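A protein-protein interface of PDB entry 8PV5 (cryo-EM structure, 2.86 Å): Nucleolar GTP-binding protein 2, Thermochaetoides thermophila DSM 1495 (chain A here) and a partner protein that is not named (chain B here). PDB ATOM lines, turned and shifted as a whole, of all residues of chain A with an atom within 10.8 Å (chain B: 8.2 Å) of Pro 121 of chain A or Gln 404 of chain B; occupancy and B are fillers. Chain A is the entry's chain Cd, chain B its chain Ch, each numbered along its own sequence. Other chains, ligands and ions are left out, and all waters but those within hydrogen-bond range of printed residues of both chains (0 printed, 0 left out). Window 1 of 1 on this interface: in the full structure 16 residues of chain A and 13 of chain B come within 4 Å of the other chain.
The side-chain amide nitrogen (NE2) of Gln 404 of chain B is in hydrogen-bond range of the backbone carbonyl oxygen (O) of Pro 121 of chain A, 3.3 Å away.
The backbone carbonyl oxygen (O) of Gly 126 of chain A lies within hydrogen-bond range of a ring nitrogen (ND1) of His 130 of chain A (2.5 Å).
The side-chain sulfur (SD) of Met 134 of chain A sits close to the side-chain amide oxygen (OE1) of Gln 131 of chain A, at 3.6 Å.
The side-chain carboxylate (OD1) of Asp 425 of chain B lies within hydrogen-bond range of a ring nitrogen (ND1) of His 403 of chain B, 2.9 Å away.
OD1 of Asp 381 of chain B sits at hydrogen-bond distance from OG1 of Thr 383 of chain B (2.5 Å).
The backbone NH (N) of Gln 404 of chain B is in hydrogen-bond range of the side-chain carboxylate (OD2) of Asp 425 of chain B (2.5 Å).
Among the printed residues, pairs that only touch across the chains: Lys 122 of chain A with Gln 404 of chain B (3.8 Å), Leu 123 of chain A with Gly 402 of chain B (3.8 Å), Leu 123 of chain A with Gln 404 of chain B (3.5 Å), Gly 126 of chain A with Gln 404 of chain B (3.4 Å), Leu 127 of chain A with Asp 381 of chain B (3.9 Å), Leu 127 of chain A with Phe 382 of chain B (3.7 Å), Leu 127 of chain A with His 403 of chain B (3.99 Å), His 130 of chain A with Phe 382 of chain B (3.4 Å), Met 134 of chain A with Asp 381 of chain B (3.4 Å) and Met 134 of chain A with Phe 382 of chain B (3.5 Å).
Of the 17 printed residues of chain B, 5 touch a printed residue of chain A.
Printed residues of chain B that touch a printed residue of chain A: Asp 381, Phe 382, Gly 402, His 403 and Gln 404.
Along chain B the printed residues that touch a printed residue of chain A span positions 381 to 404.
Of the 19 printed residues of chain A, 7 touch a printed residue of chain B.
Among the printed residues, no Asp or Glu carboxylate lies within 4 Å of a Lys or Arg side-chain nitrogen of the other chain.
No residue of chain B comes within 4 Å of Gly 120 of chain A.
Pro 121 of chain A touches one residue of chain B.
Of the printed residues of chain B, Leu 123 of chain A touches Gly 402 and Gln 404.
Lys 129 of chain A touches none of the printed residues of chain B.
Of the printed residues of chain A, Asp 381 of chain B touches Leu 127 (3.9 Å) and Met 134 (3.4 Å).
Of chain A, only Leu 123 (3.8 Å) comes within 4 Å of Gly 402 of chain B.
Of the printed residues of chain A, His 403 of chain B touches Leu 127.
Gln 404 of chain B touches four residues of chain A.
No residue of chain A comes within 4 Å of Asn 405 of chain B.
No residue of chain A comes within 4 Å of Asp 425 of chain B.
Ser 427 of chain B touches none of the printed residues of chain A.
The nearest residue of chain B that does not touch Pro 121 of chain A is Gly 402 of chain B (6.5 Å).
The nearest residue of chain A that does not touch Gln 404 of chain B is His 130 of chain A (4.4 Å).
The nearest printed residue of chain B that does not touch Leu 123 of chain A is Leu 401 of chain B (4.1 Å).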
ATOM      1  N   MET A 114      -2.781 -13.322   9.892  1.00  0.00           N
ATOM      2  CA  MET A 114      -2.453 -13.849  11.214  1.00  0.00           C
ATOM      3  C   MET A 114      -3.393 -13.326  12.290  1.00  0.00           C
ATOM      4  O   MET A 114      -3.627 -14.009  13.295  1.00  0.00           O
ATOM      5  CB  MET A 114      -1.012 -13.487  11.560  1.00  0.00           C
ATOM      6  CG  MET A 114       0.024 -14.323  10.837  1.00  0.00           C
ATOM      7  SD  MET A 114       0.228 -15.960  11.548  1.00  0.00           S
ATOM      8  CE  MET A 114       0.201 -15.553  13.289  1.00  0.00           C
ATOM      9  N   SER A 115      -3.944 -12.124  12.097  1.00  0.00           N
ATOM     10  CA  SER A 115      -4.864 -11.555  13.073  1.00  0.00           C
ATOM     11  C   SER A 115      -6.173 -12.326  13.147  1.00  0.00           C
ATOM     12  O   SER A 115      -6.807 -12.343  14.206  1.00  0.00           O
ATOM     13  CB  SER A 115      -5.151 -10.089  12.745  1.00  0.00           C
ATOM     14  OG  SER A 115      -5.870  -9.971  11.531  1.00  0.00           O
ATOM     15  N   LEU A 116      -6.590 -12.961  12.054  1.00  0.00           N
ATOM     16  CA  LEU A 116      -7.807 -13.757  12.038  1.00  0.00           C
ATOM     17  C   LEU A 116      -7.565 -15.216  12.399  1.00  0.00           C
ATOM     18  O   LEU A 116      -8.528 -15.983  12.486  1.00  0.00           O
ATOM     19  CB  LEU A 116      -8.479 -13.678  10.664  1.00  0.00           C
ATOM     20  CG  LEU A 116      -8.703 -12.286  10.076  1.00  0.00           C
ATOM     21  CD1 LEU A 116      -9.126 -12.383   8.621  1.00  0.00           C
ATOM     22  CD2 LEU A 116      -9.734 -11.527  10.886  1.00  0.00           C
ATOM     23  N   ILE A 117      -6.312 -15.615  12.620  1.00  0.00           N
ATOM     24  CA  ILE A 117      -5.967 -16.997  12.925  1.00  0.00           C
ATOM     25  C   ILE A 117      -5.504 -17.167  14.366  1.00  0.00           C
ATOM     26  O   ILE A 117      -5.928 -18.110  15.047  1.00  0.00           O
ATOM     27  CB  ILE A 117      -4.902 -17.538  11.941  1.00  0.00           C
ATOM     28  CG1 ILE A 117      -5.412 -17.446  10.505  1.00  0.00           C
ATOM     29  CG2 ILE A 117      -4.532 -18.978  12.269  1.00  0.00           C
ATOM     30  CD1 ILE A 117      -4.384 -17.819   9.462  1.00  0.00           C
ATOM     31  N   ARG A 118      -4.652 -16.265  14.858  1.00  0.00           N
ATOM     32  CA  ARG A 118      -4.123 -16.404  16.210  1.00  0.00           C
ATOM     33  C   ARG A 118      -5.221 -16.183  17.246  1.00  0.00           C
ATOM     34  O   ARG A 118      -6.198 -15.467  17.007  1.00  0.00           O
ATOM     35  CB  ARG A 118      -2.966 -15.425  16.444  1.00  0.00           C
ATOM     36  CG  ARG A 118      -3.378 -13.964  16.516  1.00  0.00           C
ATOM     37  CD  ARG A 118      -2.223 -13.052  16.902  1.00  0.00           C
ATOM     38  NE  ARG A 118      -1.172 -12.998  15.892  1.00  0.00           N
ATOM     39  CZ  ARG A 118      -0.795 -11.887  15.271  1.00  0.00           C
ATOM     40  NH1 ARG A 118      -1.385 -10.725  15.509  1.00  0.00           N
ATOM     41  NH2 ARG A 118       0.199 -11.941  14.389  1.00  0.00           N
ATOM     42  N   ASP A 119      -5.071 -16.831  18.400  1.00  0.00           N
ATOM     43  CA  ASP A 119      -6.094 -16.743  19.430  1.00  0.00           C
ATOM     44  C   ASP A 119      -6.087 -15.370  20.098  1.00  0.00           C
ATOM     45  O   ASP A 119      -5.103 -14.628  20.058  1.00  0.00           O
ATOM     46  CB  ASP A 119      -5.938 -17.868  20.466  1.00  0.00           C
ATOM     47  CG  ASP A 119      -4.612 -17.823  21.240  1.00  0.00           C
ATOM     48  OD1 ASP A 119      -3.746 -16.961  20.986  1.00  0.00           O
ATOM     49  OD2 ASP A 119      -4.447 -18.671  22.144  1.00  0.00           O
ATOM     50  N   GLY A 120      -7.217 -15.037  20.707  1.00  0.00           N
ATOM     51  CA  GLY A 120      -7.370 -13.770  21.379  1.00  0.00           C
ATOM     52  C   GLY A 120      -6.586 -13.713  22.669  1.00  0.00           C
ATOM     53  O   GLY A 120      -6.117 -14.729  23.209  1.00  0.00           O
ATOM     54  N   PRO A 121      -6.419 -12.498  23.185  1.00  0.00           N
ATOM     55  CA  PRO A 121      -5.716 -12.331  24.459  1.00  0.00           C
ATOM     56  C   PRO A 121      -6.558 -12.825  25.625  1.00  0.00           C
ATOM     57  O   PRO A 121      -7.745 -13.128  25.489  1.00  0.00           O
ATOM     58  CB  PRO A 121      -5.485 -10.818  24.542  1.00  0.00           C
ATOM     59  CG  PRO A 121      -6.588 -10.235  23.728  1.00  0.00           C
ATOM     60  CD  PRO A 121      -6.831 -11.208  22.608  1.00  0.00           C
ATOM     61  N   LYS A 122      -5.908 -12.921  26.782  1.00  0.00           N
ATOM     62  CA  LYS A 122      -6.598 -13.342  27.993  1.00  0.00           C
ATOM     63  C   LYS A 122      -7.622 -12.291  28.409  1.00  0.00           C
ATOM     64  O   LYS A 122      -7.450 -11.095  28.161  1.00  0.00           O
ATOM     65  CB  LYS A 122      -5.593 -13.583  29.119  1.00  0.00           C
ATOM     66  CG  LYS A 122      -4.601 -14.701  28.831  1.00  0.00           C
ATOM     67  CD  LYS A 122      -5.294 -16.050  28.703  1.00  0.00           C
ATOM     68  CE  LYS A 122      -5.806 -16.539  30.048  1.00  0.00           C
ATOM     69  NZ  LYS A 122      -6.419 -17.893  29.953  1.00  0.00           N
ATOM     70  N   LEU A 123      -8.708 -12.757  29.033  1.00  0.00           N
ATOM     71  CA  LEU A 123      -9.811 -11.863  29.373  1.00  0.00           C
ATOM     72  C   LEU A 123      -9.413 -10.876  30.464  1.00  0.00           C
ATOM     73  O   LEU A 123      -9.885  -9.731  30.475  1.00  0.00           O
ATOM     74  CB  LEU A 123     -11.043 -12.687  29.768  1.00  0.00           C
ATOM     75  CG  LEU A 123     -11.079 -13.657  30.959  1.00  0.00           C
ATOM     76  CD1 LEU A 123     -11.365 -12.986  32.306  1.00  0.00           C
ATOM     77  CD2 LEU A 123     -12.083 -14.774  30.692  1.00  0.00           C
ATOM     78  N   GLU A 124      -8.538 -11.297  31.383  1.00  0.00           N
ATOM     79  CA  GLU A 124      -8.042 -10.394  32.416  1.00  0.00           C
ATOM     80  C   GLU A 124      -7.286  -9.226  31.796  1.00  0.00           C
ATOM     81  O   GLU A 124      -7.508  -8.064  32.154  1.00  0.00           O
ATOM     82  CB  GLU A 124      -7.142 -11.153  33.396  1.00  0.00           C
ATOM     83  CG  GLU A 124      -7.848 -12.199  34.252  1.00  0.00           C
ATOM     84  CD  GLU A 124      -8.031 -13.529  33.541  1.00  0.00           C
ATOM     85  OE1 GLU A 124      -7.553 -13.668  32.395  1.00  0.00           O
ATOM     86  OE2 GLU A 124      -8.656 -14.435  34.131  1.00  0.00           O
ATOM     87  N   ASP A 125      -6.419  -9.520  30.825  1.00  0.00           N
ATOM     88  CA  ASP A 125      -5.706  -8.463  30.116  1.00  0.00           C
ATOM     89  C   ASP A 125      -6.654  -7.621  29.272  1.00  0.00           C
ATOM     90  O   ASP A 125      -6.488  -6.400  29.178  1.00  0.00           O
ATOM     91  CB  ASP A 125      -4.604  -9.067  29.245  1.00  0.00           C
ATOM     92  CG  ASP A 125      -3.480  -9.669  30.063  1.00  0.00           C
ATOM     93  OD1 ASP A 125      -3.229  -9.178  31.183  1.00  0.00           O
ATOM     94  OD2 ASP A 125      -2.845 -10.632  29.584  1.00  0.00           O
ATOM     95  N   GLY A 126      -7.654  -8.255  28.653  1.00  0.00           N
ATOM     96  CA  GLY A 126      -8.583  -7.518  27.808  1.00  0.00           C
ATOM     97  C   GLY A 126      -9.422  -6.518  28.581  1.00  0.00           C
ATOM     98  O   GLY A 126      -9.734  -5.436  28.079  1.00  0.00           O
ATOM     99  N   LEU A 127      -9.803  -6.868  29.810  1.00  0.00           N
ATOM    100  CA  LEU A 127     -10.467  -5.895  30.674  1.00  0.00           C
ATOM    101  C   LEU A 127      -9.484  -4.889  31.267  1.00  0.00           C
ATOM    102  O   LEU A 127      -9.845  -3.722  31.470  1.00  0.00           O
ATOM    103  CB  LEU A 127     -11.252  -6.597  31.786  1.00  0.00           C
ATOM    104  CG  LEU A 127     -12.638  -7.222  31.544  1.00  0.00           C
ATOM    105  CD1 LEU A 127     -13.645  -6.103  31.324  1.00  0.00           C
ATOM    106  CD2 LEU A 127     -12.726  -8.231  30.402  1.00  0.00           C
ATOM    107  N   LYS A 128      -8.251  -5.317  31.561  1.00  0.00           N
ATOM    108  CA  LYS A 128      -7.287  -4.425  32.201  1.00  0.00           C
ATOM    109  C   LYS A 128      -6.831  -3.319  31.256  1.00  0.00           C
ATOM    110  O   LYS A 128      -6.541  -2.201  31.700  1.00  0.00           O
ATOM    111  CB  LYS A 128      -6.092  -5.233  32.706  1.00  0.00           C
ATOM    112  CG  LYS A 128      -5.117  -4.447  33.568  1.00  0.00           C
ATOM    113  CD  LYS A 128      -4.041  -5.349  34.150  1.00  0.00           C
ATOM    114  CE  LYS A 128      -3.056  -5.793  33.082  1.00  0.00           C
ATOM    115  NZ  LYS A 128      -2.269  -4.647  32.550  1.00  0.00           N
ATOM    116  N   LYS A 129      -6.764  -3.606  29.951  1.00  0.00           N
ATOM    117  CA  LYS A 129      -6.397  -2.569  28.990  1.00  0.00           C
ATOM    118  C   LYS A 129      -7.445  -1.470  28.888  1.00  0.00           C
ATOM    119  O   LYS A 129      -7.112  -0.350  28.482  1.00  0.00           O
ATOM    120  CB  LYS A 129      -6.162  -3.156  27.591  1.00  0.00           C
ATOM    121  CG  LYS A 129      -5.050  -4.205  27.418  1.00  0.00           C
ATOM    122  CD  LYS A 129      -3.619  -3.666  27.532  1.00  0.00           C
ATOM    123  CE  LYS A 129      -3.036  -3.790  28.938  1.00  0.00           C
ATOM    124  NZ  LYS A 129      -1.616  -3.358  28.983  1.00  0.00           N
ATOM    125  N   HIS A 130      -8.697  -1.753  29.243  1.00  0.00           N
ATOM    126  CA  HIS A 130      -9.775  -0.795  29.059  1.00  0.00           C
ATOM    127  C   HIS A 130     -10.404  -0.294  30.351  1.00  0.00           C
ATOM    128  O   HIS A 130     -11.321   0.530  30.274  1.00  0.00           O
ATOM    129  CB  HIS A 130     -10.876  -1.392  28.171  1.00  0.00           C
ATOM    130  CG  HIS A 130     -10.369  -1.976  26.889  1.00  0.00           C
ATOM    131  ND1 HIS A 130      -9.853  -3.251  26.803  1.00  0.00           N
ATOM    132  CD2 HIS A 130     -10.299  -1.457  25.641  1.00  0.00           C
ATOM    133  CE1 HIS A 130      -9.488  -3.493  25.557  1.00  0.00           C
ATOM    134  NE2 HIS A 130      -9.747  -2.421  24.831  1.00  0.00           N
ATOM    135  N   GLN A 131      -9.961  -0.776  31.522  1.00  0.00           N
ATOM    136  CA  GLN A 131     -10.530  -0.309  32.792  1.00  0.00           C
ATOM    137  C   GLN A 131     -10.380   1.199  32.970  1.00  0.00           C
ATOM    138  O   GLN A 131     -11.313   1.870  33.432  1.00  0.00           O
ATOM    139  CB  GLN A 131      -9.875  -1.031  33.972  1.00  0.00           C
ATOM    140  CG  GLN A 131     -10.451  -2.396  34.294  1.00  0.00           C
ATOM    141  CD  GLN A 131     -11.902  -2.332  34.716  1.00  0.00           C
ATOM    142  OE1 GLN A 131     -12.794  -2.745  33.976  1.00  0.00           O
ATOM    143  NE2 GLN A 131     -12.148  -1.811  35.911  1.00  0.00           N
ATOM    144  N   MET A 134     -12.812   3.005  30.675  1.00  0.00           N
ATOM    145  CA  MET A 134     -14.158   2.850  31.223  1.00  0.00           C
ATOM    146  C   MET A 134     -14.398   3.788  32.395  1.00  0.00           C
ATOM    147  O   MET A 134     -15.478   4.374  32.503  1.00  0.00           O
ATOM    148  CB  MET A 134     -14.398   1.414  31.680  1.00  0.00           C
ATOM    149  CG  MET A 134     -14.446   0.383  30.592  1.00  0.00           C
ATOM    150  SD  MET A 134     -14.720  -1.241  31.305  1.00  0.00           S
ATOM    151  CE  MET A 134     -14.620  -2.233  29.833  1.00  0.00           C
ATOM    152  N   ASP B 381     -19.563  -2.167  29.628  1.00  0.00           N
ATOM    153  CA  ASP B 381     -18.355  -2.415  30.401  1.00  0.00           C
ATOM    154  C   ASP B 381     -17.749  -3.783  30.115  1.00  0.00           C
ATOM    155  O   ASP B 381     -17.063  -4.331  30.984  1.00  0.00           O
ATOM    156  CB  ASP B 381     -18.633  -2.253  31.903  1.00  0.00           C
ATOM    157  CG  ASP B 381     -19.713  -3.197  32.429  1.00  0.00           C
ATOM    158  OD1 ASP B 381     -20.204  -4.075  31.695  1.00  0.00           O
ATOM    159  OD2 ASP B 381     -20.066  -3.071  33.617  1.00  0.00           O
ATOM    160  N   PHE B 382     -18.046  -4.354  28.940  1.00  0.00           N
ATOM    161  CA  PHE B 382     -17.518  -5.608  28.393  1.00  0.00           C
ATOM    162  C   PHE B 382     -18.097  -6.826  29.100  1.00  0.00           C
ATOM    163  O   PHE B 382     -17.730  -7.959  28.772  1.00  0.00           O
ATOM    164  CB  PHE B 382     -15.983  -5.702  28.436  1.00  0.00           C
ATOM    165  CG  PHE B 382     -15.249  -4.741  27.519  1.00  0.00           C
ATOM    166  CD1 PHE B 382     -13.883  -4.874  27.347  1.00  0.00           C
ATOM    167  CD2 PHE B 382     -15.897  -3.710  26.852  1.00  0.00           C
ATOM    168  CE1 PHE B 382     -13.182  -4.011  26.532  1.00  0.00           C
ATOM    169  CE2 PHE B 382     -15.201  -2.841  26.038  1.00  0.00           C
ATOM    170  CZ  PHE B 382     -13.843  -2.995  25.874  1.00  0.00           C
ATOM    171  N   THR B 383     -19.001  -6.630  30.060  1.00  0.00           N
ATOM    172  CA  THR B 383     -19.433  -7.702  30.942  1.00  0.00           C
ATOM    173  C   THR B 383     -20.939  -7.887  30.847  1.00  0.00           C
ATOM    174  O   THR B 383     -21.662  -7.112  30.199  1.00  0.00           O
ATOM    175  CB  THR B 383     -19.058  -7.429  32.405  1.00  0.00           C
ATOM    176  OG1 THR B 383     -19.784  -6.289  32.878  1.00  0.00           O
ATOM    177  CG2 THR B 383     -17.575  -7.153  32.536  1.00  0.00           C
ATOM    178  N   LEU B 401     -18.163 -13.098  32.043  1.00  0.00           N
ATOM    179  CA  LEU B 401     -16.873 -12.484  31.767  1.00  0.00           C
ATOM    180  C   LEU B 401     -16.189 -13.250  30.647  1.00  0.00           C
ATOM    181  O   LEU B 401     -16.176 -14.483  30.633  1.00  0.00           O
ATOM    182  CB  LEU B 401     -15.970 -12.505  33.009  1.00  0.00           C
ATOM    183  CG  LEU B 401     -16.260 -11.603  34.204  1.00  0.00           C
ATOM    184  CD1 LEU B 401     -15.365 -11.985  35.364  1.00  0.00           C
ATOM    185  CD2 LEU B 401     -16.014 -10.170  33.824  1.00  0.00           C
ATOM    186  N   GLY B 402     -15.586 -12.511  29.722  1.00  0.00           N
ATOM    187  CA  GLY B 402     -14.854 -13.106  28.627  1.00  0.00           C
ATOM    188  C   GLY B 402     -14.953 -12.366  27.312  1.00  0.00           C
ATOM    189  O   GLY B 402     -14.152 -12.635  26.409  1.00  0.00           O
ATOM    190  N   HIS B 403     -15.905 -11.452  27.176  1.00  0.00           N
ATOM    191  CA  HIS B 403     -15.988 -10.646  25.970  1.00  0.00           C
ATOM    192  C   HIS B 403     -14.905  -9.576  25.989  1.00  0.00           C
ATOM    193  O   HIS B 403     -14.701  -8.895  26.998  1.00  0.00           O
ATOM    194  CB  HIS B 403     -17.370 -10.005  25.861  1.00  0.00           C
ATOM    195  CG  HIS B 403     -18.311 -10.749  24.963  1.00  0.00           C
ATOM    196  ND1 HIS B 403     -18.162 -10.787  23.594  1.00  0.00           N
ATOM    197  CD2 HIS B 403     -19.406 -11.492  25.244  1.00  0.00           C
ATOM    198  CE1 HIS B 403     -19.130 -11.517  23.069  1.00  0.00           C
ATOM    199  NE2 HIS B 403     -19.898 -11.956  24.048  1.00  0.00           N
ATOM    200  N   GLN B 404     -14.201  -9.436  24.872  1.00  0.00           N
ATOM    201  CA  GLN B 404     -13.100  -8.490  24.771  1.00  0.00           C
ATOM    202  C   GLN B 404     -13.548  -7.104  24.335  1.00  0.00           C
ATOM    203  O   GLN B 404     -12.710  -6.203  24.224  1.00  0.00           O
ATOM    204  CB  GLN B 404     -12.040  -9.018  23.802  1.00  0.00           C
ATOM    205  CG  GLN B 404     -11.578 -10.424  24.115  1.00  0.00           C
ATOM    206  CD  GLN B 404     -10.516 -10.457  25.191  1.00  0.00           C
ATOM    207  OE1 GLN B 404      -9.680  -9.559  25.281  1.00  0.00           O
ATOM    208  NE2 GLN B 404     -10.544 -11.494  26.017  1.00  0.00           N
ATOM    209  N   ASN B 405     -14.838  -6.911  24.080  1.00  0.00           N
ATOM    210  CA  ASN B 405     -15.369  -5.604  23.732  1.00  0.00           C
ATOM    211  C   ASN B 405     -16.812  -5.544  24.215  1.00  0.00           C
ATOM    212  O   ASN B 405     -17.276  -6.423  24.947  1.00  0.00           O
ATOM    213  CB  ASN B 405     -15.239  -5.340  22.229  1.00  0.00           C
ATOM    214  CG  ASN B 405     -15.112  -3.868  21.904  1.00  0.00           C
ATOM    215  OD1 ASN B 405     -15.373  -3.012  22.746  1.00  0.00           O
ATOM    216  ND2 ASN B 405     -14.706  -3.564  20.679  1.00  0.00           N
ATOM    217  N   LYS B 406     -17.513  -4.481  23.818  1.00  0.00           N
ATOM    218  CA  LYS B 406     -18.877  -4.247  24.277  1.00  0.00           C
ATOM    219  C   LYS B 406     -19.813  -5.334  23.768  1.00  0.00           C
ATOM    220  O   LYS B 406     -19.645  -5.852  22.662  1.00  0.00           O
ATOM    221  CB  LYS B 406     -19.361  -2.875  23.802  1.00  0.00           C
ATOM    222  CG  LYS B 406     -18.411  -1.741  24.130  1.00  0.00           C
ATOM    223  CD  LYS B 406     -18.944  -0.410  23.631  1.00  0.00           C
ATOM    224  CE  LYS B 406     -19.036  -0.373  22.120  1.00  0.00           C
ATOM    225  NZ  LYS B 406     -17.696  -0.495  21.490  1.00  0.00           N
ATOM    226  N   VAL B 407     -20.793  -5.693  24.590  1.00  0.00           N
ATOM    227  CA  VAL B 407     -21.755  -6.730  24.243  1.00  0.00           C
ATOM    228  C   VAL B 407     -23.033  -6.034  23.801  1.00  0.00           C
ATOM    229  O   VAL B 407     -23.606  -5.235  24.549  1.00  0.00           O
ATOM    230  CB  VAL B 407     -22.018  -7.677  25.423  1.00  0.00           C
ATOM    231  CG1 VAL B 407     -23.019  -8.743  25.019  1.00  0.00           C
ATOM    232  CG2 VAL B 407     -20.729  -8.290  25.917  1.00  0.00           C
ATOM    233  N   GLY B 423     -21.017  -9.763  20.651  1.00  0.00           N
ATOM    234  CA  GLY B 423     -20.114  -8.739  21.123  1.00  0.00           C
ATOM    235  C   GLY B 423     -19.513  -7.939  19.981  1.00  0.00           C
ATOM    236  O   GLY B 423     -19.610  -8.308  18.808  1.00  0.00           O
ATOM    237  N   TRP B 424     -18.886  -6.829  20.357  1.00  0.00           N
ATOM    238  CA  TRP B 424     -18.141  -5.984  19.435  1.00  0.00           C
ATOM    239  C   TRP B 424     -16.723  -6.483  19.209  1.00  0.00           C
ATOM    240  O   TRP B 424     -15.978  -5.870  18.439  1.00  0.00           O
ATOM    241  CB  TRP B 424     -18.111  -4.542  19.947  1.00  0.00           C
ATOM    242  CG  TRP B 424     -19.409  -3.807  19.782  1.00  0.00           C
ATOM    243  CD1 TRP B 424     -20.631  -4.185  20.250  1.00  0.00           C
ATOM    244  CD2 TRP B 424     -19.605  -2.558  19.113  1.00  0.00           C
ATOM    245  NE1 TRP B 424     -21.578  -3.253  19.908  1.00  0.00           N
ATOM    246  CE2 TRP B 424     -20.974  -2.242  19.209  1.00  0.00           C
ATOM    247  CE3 TRP B 424     -18.757  -1.676  18.437  1.00  0.00           C
ATOM    248  CZ2 TRP B 424     -21.514  -1.086  18.656  1.00  0.00           C
ATOM    249  CZ3 TRP B 424     -19.295  -0.528  17.889  1.00  0.00           C
ATOM    250  CH2 TRP B 424     -20.660  -0.244  18.002  1.00  0.00           C
ATOM    251  N   ASP B 425     -16.338  -7.578  19.864  1.00  0.00           N
ATOM    252  CA  ASP B 425     -15.057  -8.232  19.645  1.00  0.00           C
ATOM    253  C   ASP B 425     -15.158  -9.346  18.612  1.00  0.00           C
ATOM    254  O   ASP B 425     -14.484 -10.374  18.752  1.00  0.00           O
ATOM    255  CB  ASP B 425     -14.507  -8.783  20.961  1.00  0.00           C
ATOM    256  CG  ASP B 425     -15.522  -9.612  21.711  1.00  0.00           C
ATOM    257  OD1 ASP B 425     -16.706  -9.603  21.322  1.00  0.00           O
ATOM    258  OD2 ASP B 425     -15.135 -10.279  22.691  1.00  0.00           O
ATOM    259  N   ASN B 426     -16.037  -9.178  17.620  1.00  0.00           N
ATOM    260  CA  ASN B 426     -16.220 -10.058  16.470  1.00  0.00           C
ATOM    261  C   ASN B 426     -16.741 -11.436  16.857  1.00  0.00           C
ATOM    262  O   ASN B 426     -16.658 -12.372  16.057  1.00  0.00           O
ATOM    263  CB  ASN B 426     -14.922 -10.218  15.665  1.00  0.00           C
ATOM    264  CG  ASN B 426     -14.434  -8.916  15.076  1.00  0.00           C
ATOM    265  OD1 ASN B 426     -15.222  -8.076  14.666  1.00  0.00           O
ATOM    266  ND2 ASN B 426     -13.120  -8.749  15.022  1.00  0.00           N
ATOM    267  N   SER B 427     -17.291 -11.594  18.060  1.00  0.00           N
ATOM    268  CA  SER B 427     -17.528 -12.919  18.608  1.00  0.00           C
ATOM    269  C   SER B 427     -18.935 -13.055  19.174  1.00  0.00           C
ATOM    270  O   SER B 427     -19.498 -12.131  19.771  1.00  0.00           O
ATOM    271  CB  SER B 427     -16.506 -13.256  19.700  1.00  0.00           C
ATOM    272  OG  SER B 427     -16.802 -12.566  20.900  1.00  0.00           O
ATOM    273  N   LYS B 429     -20.775 -15.679  21.855  1.00  0.00           N
ATOM    274  CA  LYS B 429     -20.397 -16.599  22.916  1.00  0.00           C
ATOM    275  C   LYS B 429     -21.623 -17.278  23.504  1.00  0.00           C
ATOM    276  O   LYS B 429     -22.726 -16.719  23.495  1.00  0.00           O
ATOM    277  CB  LYS B 429     -19.615 -15.880  24.015  1.00  0.00           C
ATOM    278  CG  LYS B 429     -18.207 -15.502  23.603  1.00  0.00           C
ATOM    279  CD  LYS B 429     -17.429 -14.910  24.758  1.00  0.00           C
ATOM    280  CE  LYS B 429     -15.958 -14.793  24.413  1.00  0.00           C
ATOM    281  NZ  LYS B 429     -15.730 -13.905  23.241  1.00  0.00           N
ATOM    282  N   ASN B 441     -16.941 -20.418  22.136  1.00  0.00           N
ATOM    283  CA  ASN B 441     -16.915 -19.185  21.366  1.00  0.00           C
ATOM    284  C   ASN B 441     -17.167 -19.492  19.898  1.00  0.00           C
ATOM    285  O   ASN B 441     -16.585 -20.427  19.339  1.00  0.00           O
ATOM    286  CB  ASN B 441     -15.573 -18.469  21.528  1.00  0.00           C
ATOM    287  CG  ASN B 441     -15.553 -17.111  20.857  1.00  0.00           C
ATOM    288  OD1 ASN B 441     -16.581 -16.446  20.745  1.00  0.00           O
ATOM    289  ND2 ASN B 441     -14.378 -16.693  20.405  1.00  0.00           N
